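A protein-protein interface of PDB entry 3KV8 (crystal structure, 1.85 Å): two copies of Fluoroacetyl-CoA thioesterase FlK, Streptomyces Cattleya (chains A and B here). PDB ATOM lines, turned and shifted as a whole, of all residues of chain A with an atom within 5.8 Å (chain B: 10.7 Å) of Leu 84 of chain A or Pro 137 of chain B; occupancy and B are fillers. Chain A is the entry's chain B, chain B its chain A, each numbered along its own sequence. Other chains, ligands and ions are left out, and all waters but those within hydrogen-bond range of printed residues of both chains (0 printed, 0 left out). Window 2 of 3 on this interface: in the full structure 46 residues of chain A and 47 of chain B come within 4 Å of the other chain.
Hydrophobic or aromatic side chains of chain A within 4 Å of the printed part of chain B: Phe 15, Pro 81 and Leu 84. Of the 9 printed residues of chain B, 5 touch a printed residue of chain A. Hydrophobic or aromatic side chains of chain B within 4 Å of the printed part of chain A: Tyr 27, Val 132 and Pro 137. Among the printed residues, Asp or Glu carboxylates within 4 Å of a Lys or Arg side-chain nitrogen of the other chain: Asp 108 of chain A with Lys 135 of chain B (2.7 Å).
The side-chain amino group (NZ) of Lys 135 of chain B sits at hydrogen-bond distance from the backbone carbonyl oxygen (O) of Ala 79 of chain A, at 2.9 Å. The side-chain carboxylate of Asp 108 of chain A is in salt-bridge range of the side-chain amino group of Lys 135 of chain B (2.7 Å).
Phe 15 of chain A touches Tyr 27 of chain B. CG2 of Val 132 of chain B touches CB of Pro 81 of chain A (3.8 Å). O of Lys 135 of chain B touches CG of Pro 81 of chain A, 3.9 Å away. Pro 81 of chain A touches Thr 136 of chain B (CG to OG1, 3.4 Å). CD of Pro 137 of chain B touches O of Pro 82 of chain A (3.9 Å). C of Gly 83 of chain A touches CG of Pro 137 of chain B, at 3.9 Å. Lys 135 of chain B touches Leu 84 of chain A. Leu 84 of chain A touches Pro 137 of chain B (CD2 to CG, 3.7 Å).
The backbone carbonyl oxygen (O) of Leu 84 of chain A lies within hydrogen-bond range of the backbone NH (N) of Val 17 of chain A (2.9 Å). The side-chain hydroxyl of Thr 80 of chain A lies within hydrogen-bond range of the side-chain carboxylate of Asp 108 of chain A. N of Val 86 of chain A sits at hydrogen-bond distance from O of Phe 15 of chain A, 2.8 Å away. OD1 of Asp 108 of chain A is in hydrogen-bond range of N of Val 110 of chain A (3.0 Å). The side-chain hydroxyl (OG1) of Thr 136 of chain B lies within hydrogen-bond range of the backbone carbonyl oxygen (O) of Val 132 of chain B, at 2.7 Å. O of Val 17 of chain A is in hydrogen-bond range of N of Gly 83 of chain A (2.8 Å).
No position is printed for both chains.
Leu 84 of chain A touches just these residues of chain B: Lys 135 (3.4 Å) and Pro 137 (3.7 Å). Printed residues of chain A within 4 Å of Pro 137 of chain B: Pro 82, Gly 83 and Leu 84. No residue of chain B comes within 4 Å of Val 16 of chain A. Pro 81 of chain A touches three residues of chain B. Printed residues of chain B within 4 Å of Asp 108 of chain A: Lys 135. Printed residues of chain B within 4 Å of Ala 79 of chain A: Lys 135. Printed residues of chain A within 4 Å of Val 132 of chain B: Pro 81 (3.8 Å). Printed residues of chain A within 4 Å of Thr 136 of chain B: Pro 81. Printed residues of chain A within 4 Å of Tyr 27 of chain B: Phe 15. Lys 131 of chain B touches none of the printed residues of chain A. Arg 133 of chain B touches none of the printed residues of chain A. The nearest residue of chain A that does not touch Pro 137 of chain B is Pro 81 of chain A (4.7 Å). The nearest printed residue of chain A that does not touch Tyr 27 of chain B is Val 17 of chain A (7.2 Å).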
ATOM      1  N   PHE A  15      -5.024  25.598 -20.068  1.00  0.00           N
ATOM      2  CA  PHE A  15      -5.865  25.916 -18.956  1.00  0.00           C
ATOM      3  C   PHE A  15      -5.907  24.712 -18.066  1.00  0.00           C
ATOM      4  O   PHE A  15      -6.363  23.621 -18.496  1.00  0.00           O
ATOM      5  CB  PHE A  15      -7.289  26.231 -19.445  1.00  0.00           C
ATOM      6  CG  PHE A  15      -8.255  26.557 -18.307  1.00  0.00           C
ATOM      7  CD1 PHE A  15      -8.101  27.748 -17.532  1.00  0.00           C
ATOM      8  CD2 PHE A  15      -9.287  25.649 -17.977  1.00  0.00           C
ATOM      9  CE1 PHE A  15      -9.045  28.011 -16.459  1.00  0.00           C
ATOM     10  CE2 PHE A  15     -10.179  25.893 -16.937  1.00  0.00           C
ATOM     11  CZ  PHE A  15     -10.096  27.077 -16.195  1.00  0.00           C
ATOM     12  N   VAL A  16      -5.400  24.878 -16.840  1.00  0.00           N
ATOM     13  CA  VAL A  16      -5.505  23.821 -15.814  1.00  0.00           C
ATOM     14  C   VAL A  16      -6.943  23.813 -15.254  1.00  0.00           C
ATOM     15  O   VAL A  16      -7.452  24.823 -14.757  1.00  0.00           O
ATOM     16  CB  VAL A  16      -4.507  24.018 -14.633  1.00  0.00           C
ATOM     17  CG1 VAL A  16      -4.698  22.880 -13.524  1.00  0.00           C
ATOM     18  CG2 VAL A  16      -3.055  24.085 -15.139  1.00  0.00           C
ATOM     19  N   VAL A  17      -7.597  22.666 -15.376  1.00  0.00           N
ATOM     20  CA  VAL A  17      -9.018  22.566 -14.973  1.00  0.00           C
ATOM     21  C   VAL A  17      -9.128  22.615 -13.436  1.00  0.00           C
ATOM     22  O   VAL A  17      -8.652  21.732 -12.759  1.00  0.00           O
ATOM     23  CB  VAL A  17      -9.637  21.251 -15.542  1.00  0.00           C
ATOM     24  CG1 VAL A  17     -11.147  21.154 -15.151  1.00  0.00           C
ATOM     25  CG2 VAL A  17      -9.532  21.255 -17.092  1.00  0.00           C
ATOM     26  N   ALA A  79     -13.443  12.261 -21.213  1.00  0.00           N
ATOM     27  CA  ALA A  79     -13.697  13.095 -20.030  1.00  0.00           C
ATOM     28  C   ALA A  79     -12.428  13.522 -19.271  1.00  0.00           C
ATOM     29  O   ALA A  79     -11.419  12.799 -19.242  1.00  0.00           O
ATOM     30  CB  ALA A  79     -14.686  12.431 -19.044  1.00  0.00           C
ATOM     31  N   THR A  80     -12.518  14.668 -18.606  1.00  0.00           N
ATOM     32  CA  THR A  80     -11.355  15.276 -18.007  1.00  0.00           C
ATOM     33  C   THR A  80     -11.613  15.660 -16.562  1.00  0.00           C
ATOM     34  O   THR A  80     -12.448  16.512 -16.277  1.00  0.00           O
ATOM     35  CB  THR A  80     -10.917  16.575 -18.780  1.00  0.00           C
ATOM     36  OG1 THR A  80     -10.586  16.247 -20.103  1.00  0.00           O
ATOM     37  CG2 THR A  80      -9.715  17.201 -18.086  1.00  0.00           C
ATOM     38  N   PRO A  81     -10.865  15.052 -15.599  1.00  0.00           N
ATOM     39  CA  PRO A  81     -11.049  15.459 -14.218  1.00  0.00           C
ATOM     40  C   PRO A  81     -10.260  16.739 -13.902  1.00  0.00           C
ATOM     41  O   PRO A  81      -9.292  17.046 -14.625  1.00  0.00           O
ATOM     42  CB  PRO A  81     -10.429  14.293 -13.421  1.00  0.00           C
ATOM     43  CG  PRO A  81      -9.354  13.815 -14.269  1.00  0.00           C
ATOM     44  CD  PRO A  81      -9.825  14.028 -15.759  1.00  0.00           C
ATOM     45  N   PRO A  82     -10.634  17.432 -12.820  1.00  0.00           N
ATOM     46  CA  PRO A  82      -9.852  18.613 -12.399  1.00  0.00           C
ATOM     47  C   PRO A  82      -8.369  18.270 -12.214  1.00  0.00           C
ATOM     48  O   PRO A  82      -8.007  17.139 -11.789  1.00  0.00           O
ATOM     49  CB  PRO A  82     -10.470  18.995 -11.032  1.00  0.00           C
ATOM     50  CG  PRO A  82     -11.908  18.532 -11.121  1.00  0.00           C
ATOM     51  CD  PRO A  82     -11.790  17.195 -11.944  1.00  0.00           C
ATOM     52  N   GLY A  83      -7.512  19.229 -12.544  1.00  0.00           N
ATOM     53  CA  GLY A  83      -6.069  19.049 -12.324  1.00  0.00           C
ATOM     54  C   GLY A  83      -5.293  18.774 -13.587  1.00  0.00           C
ATOM     55  O   GLY A  83      -4.074  19.123 -13.638  1.00  0.00           O
ATOM     56  N   LEU A  84      -5.935  18.175 -14.606  1.00  0.00           N
ATOM     57  CA  LEU A  84      -5.330  18.131 -15.955  1.00  0.00           C
ATOM     58  C   LEU A  84      -5.284  19.480 -16.669  1.00  0.00           C
ATOM     59  O   LEU A  84      -6.120  20.361 -16.411  1.00  0.00           O
ATOM     60  CB  LEU A  84      -5.942  17.065 -16.876  1.00  0.00           C
ATOM     61  CG  LEU A  84      -5.789  15.604 -16.339  1.00  0.00           C
ATOM     62  CD1 LEU A  84      -6.435  14.614 -17.279  1.00  0.00           C
ATOM     63  CD2 LEU A  84      -4.324  15.271 -16.263  1.00  0.00           C
ATOM     64  N   THR A  85      -4.295  19.650 -17.533  1.00  0.00           N
ATOM     65  CA  THR A  85      -4.263  20.830 -18.424  1.00  0.00           C
ATOM     66  C   THR A  85      -5.001  20.567 -19.773  1.00  0.00           C
ATOM     67  O   THR A  85      -4.614  19.683 -20.534  1.00  0.00           O
ATOM     68  CB  THR A  85      -2.801  21.272 -18.665  1.00  0.00           C
ATOM     69  OG1 THR A  85      -2.202  21.546 -17.395  1.00  0.00           O
ATOM     70  CG2 THR A  85      -2.777  22.619 -19.555  1.00  0.00           C
ATOM     71  N   VAL A  86      -6.061  21.329 -20.040  1.00  0.00           N
ATOM     72  CA  VAL A  86      -6.679  21.330 -21.347  1.00  0.00           C
ATOM     73  C   VAL A  86      -6.016  22.360 -22.263  1.00  0.00           C
ATOM     74  O   VAL A  86      -5.965  23.554 -21.939  1.00  0.00           O
ATOM     75  CB  VAL A  86      -8.211  21.522 -21.282  1.00  0.00           C
ATOM     76  CG1 VAL A  86      -8.764  21.565 -22.731  1.00  0.00           C
ATOM     77  CG2 VAL A  86      -8.808  20.378 -20.393  1.00  0.00           C
ATOM     78  N   ASP A 108      -6.385  16.921 -23.286  1.00  0.00           N
ATOM     79  CA  ASP A 108      -6.108  17.158 -21.873  1.00  0.00           C
ATOM     80  C   ASP A 108      -4.750  16.638 -21.369  1.00  0.00           C
ATOM     81  O   ASP A 108      -4.548  16.458 -20.163  1.00  0.00           O
ATOM     82  CB  ASP A 108      -7.227  16.677 -20.944  1.00  0.00           C
ATOM     83  CG  ASP A 108      -7.473  15.149 -21.047  1.00  0.00           C
ATOM     84  OD1 ASP A 108      -6.611  14.442 -21.584  1.00  0.00           O
ATOM     85  OD2 ASP A 108      -8.542  14.696 -20.602  1.00  0.00           O
ATOM     86  N   VAL A 110      -3.753  13.739 -22.068  1.00  0.00           N
ATOM     87  CA  VAL A 110      -3.931  12.254 -22.035  1.00  0.00           C
ATOM     88  C   VAL A 110      -4.651  11.817 -23.250  1.00  0.00           C
ATOM     89  O   VAL A 110      -4.131  11.002 -24.014  1.00  0.00           O
ATOM     90  CB  VAL A 110      -4.634  11.784 -20.729  1.00  0.00           C
ATOM     91  CG1 VAL A 110      -4.894  10.276 -20.759  1.00  0.00           C
ATOM     92  CG2 VAL A 110      -3.815  12.247 -19.543  1.00  0.00           C
ATOM     93  N   TYR B  27     -16.390  32.160 -17.225  1.00  0.00           N
ATOM     94  CA  TYR B  27     -14.966  32.174 -16.975  1.00  0.00           C
ATOM     95  C   TYR B  27     -14.588  33.500 -16.255  1.00  0.00           C
ATOM     96  O   TYR B  27     -14.124  34.463 -16.907  1.00  0.00           O
ATOM     97  CB  TYR B  27     -14.186  32.049 -18.295  1.00  0.00           C
ATOM     98  CG  TYR B  27     -14.032  30.631 -18.654  1.00  0.00           C
ATOM     99  CD1 TYR B  27     -13.094  29.836 -18.015  1.00  0.00           C
ATOM    100  CD2 TYR B  27     -14.945  30.037 -19.542  1.00  0.00           C
ATOM    101  CE1 TYR B  27     -12.946  28.505 -18.324  1.00  0.00           C
ATOM    102  CE2 TYR B  27     -14.844  28.699 -19.863  1.00  0.00           C
ATOM    103  CZ  TYR B  27     -13.847  27.924 -19.268  1.00  0.00           C
ATOM    104  OH  TYR B  27     -13.773  26.576 -19.534  1.00  0.00           O
ATOM    105  N   ALA B 130     -14.184   4.905 -12.534  1.00  0.00           N
ATOM    106  CA  ALA B 130     -12.900   4.246 -12.425  1.00  0.00           C
ATOM    107  C   ALA B 130     -11.956   4.676 -13.543  1.00  0.00           C
ATOM    108  O   ALA B 130     -10.733   4.865 -13.323  1.00  0.00           O
ATOM    109  CB  ALA B 130     -13.065   2.712 -12.460  1.00  0.00           C
ATOM    110  N   LYS B 131     -12.507   4.832 -14.735  1.00  0.00           N
ATOM    111  CA  LYS B 131     -11.694   5.285 -15.854  1.00  0.00           C
ATOM    112  C   LYS B 131     -11.162   6.683 -15.583  1.00  0.00           C
ATOM    113  O   LYS B 131     -10.004   7.002 -15.932  1.00  0.00           O
ATOM    114  CB  LYS B 131     -12.510   5.310 -17.129  1.00  0.00           C
ATOM    115  CG  LYS B 131     -12.661   3.961 -17.734  1.00  0.00           C
ATOM    116  CD  LYS B 131     -12.922   4.068 -19.234  1.00  0.00           C
ATOM    117  CE  LYS B 131     -13.599   2.803 -19.718  1.00  0.00           C
ATOM    118  NZ  LYS B 131     -13.039   1.621 -18.962  1.00  0.00           N
ATOM    119  N   VAL B 132     -12.037   7.524 -15.042  1.00  0.00           N
ATOM    120  CA  VAL B 132     -11.676   8.932 -14.783  1.00  0.00           C
ATOM    121  C   VAL B 132     -10.638   9.009 -13.658  1.00  0.00           C
ATOM    122  O   VAL B 132      -9.667   9.784 -13.755  1.00  0.00           O
ATOM    123  CB  VAL B 132     -12.910   9.834 -14.475  1.00  0.00           C
ATOM    124  CG1 VAL B 132     -13.891   9.113 -13.661  1.00  0.00           C
ATOM    125  CG2 VAL B 132     -12.523  11.120 -13.724  1.00  0.00           C
ATOM    126  N   ARG B 133     -10.845   8.210 -12.599  1.00  0.00           N
ATOM    127  CA  ARG B 133      -9.791   8.056 -11.557  1.00  0.00           C
ATOM    128  C   ARG B 133      -8.423   7.702 -12.113  1.00  0.00           C
ATOM    129  O   ARG B 133      -7.422   8.280 -11.695  1.00  0.00           O
ATOM    130  CB  ARG B 133     -10.218   7.093 -10.447  1.00  0.00           C
ATOM    131  CG  ARG B 133     -11.296   7.695  -9.596  1.00  0.00           C
ATOM    132  CD  ARG B 133     -11.369   7.048  -8.235  1.00  0.00           C
ATOM    133  NE  ARG B 133     -12.763   6.701  -7.986  1.00  0.00           N
ATOM    134  CZ  ARG B 133     -13.359   5.579  -8.409  1.00  0.00           C
ATOM    135  NH1 ARG B 133     -12.668   4.647  -9.057  1.00  0.00           N
ATOM    136  NH2 ARG B 133     -14.652   5.398  -8.151  1.00  0.00           N
ATOM    137  N   GLN B 134      -8.374   6.827 -13.108  1.00  0.00           N
ATOM    138  CA  GLN B 134      -7.088   6.440 -13.614  1.00  0.00           C
ATOM    139  C   GLN B 134      -6.321   7.529 -14.388  1.00  0.00           C
ATOM    140  O   GLN B 134      -5.105   7.408 -14.566  1.00  0.00           O
ATOM    141  CB  GLN B 134      -7.145   5.111 -14.318  1.00  0.00           C
ATOM    142  CG  GLN B 134      -7.633   5.085 -15.721  1.00  0.00           C
ATOM    143  CD  GLN B 134      -7.912   3.649 -16.131  1.00  0.00           C
ATOM    144  OE1 GLN B 134      -7.691   2.727 -15.338  1.00  0.00           O
ATOM    145  NE2 GLN B 134      -8.415   3.449 -17.352  1.00  0.00           N
ATOM    146  N   LYS B 135      -6.997   8.628 -14.749  1.00  0.00           N
ATOM    147  CA  LYS B 135      -6.297   9.732 -15.405  1.00  0.00           C
ATOM    148  C   LYS B 135      -6.283  10.995 -14.556  1.00  0.00           C
ATOM    149  O   LYS B 135      -5.930  12.072 -15.057  1.00  0.00           O
ATOM    150  CB  LYS B 135      -6.829   9.983 -16.825  1.00  0.00           C
ATOM    151  CG  LYS B 135      -8.302  10.403 -16.914  1.00  0.00           C
ATOM    152  CD  LYS B 135      -8.773  10.494 -18.406  1.00  0.00           C
ATOM    153  CE  LYS B 135      -8.517  11.894 -19.012  1.00  0.00           C
ATOM    154  NZ  LYS B 135      -8.901  12.033 -20.483  1.00  0.00           N
ATOM    155  N   THR B 136      -6.656  10.848 -13.287  1.00  0.00           N
ATOM    156  CA  THR B 136      -6.673  11.948 -12.339  1.00  0.00           C
ATOM    157  C   THR B 136      -5.270  12.067 -11.716  1.00  0.00           C
ATOM    158  O   THR B 136      -4.759  11.051 -11.231  1.00  0.00           O
ATOM    159  CB  THR B 136      -7.690  11.682 -11.222  1.00  0.00           C
ATOM    160  OG1 THR B 136      -8.993  11.519 -11.803  1.00  0.00           O
ATOM    161  CG2 THR B 136      -7.695  12.812 -10.182  1.00  0.00           C
ATOM    162  N   PRO B 137      -4.650  13.279 -11.735  1.00  0.00           N
ATOM    163  CA  PRO B 137      -3.292  13.415 -11.183  1.00  0.00           C
ATOM    164  C   PRO B 137      -3.272  13.126  -9.687  1.00  0.00           C
ATOM    165  O   PRO B 137      -4.155  13.554  -8.907  1.00  0.00           O
ATOM    166  CB  PRO B 137      -2.934  14.894 -11.448  1.00  0.00           C
ATOM    167  CG  PRO B 137      -3.810  15.294 -12.590  1.00  0.00           C
ATOM    168  CD  PRO B 137      -5.119  14.547 -12.331  1.00  0.00           C
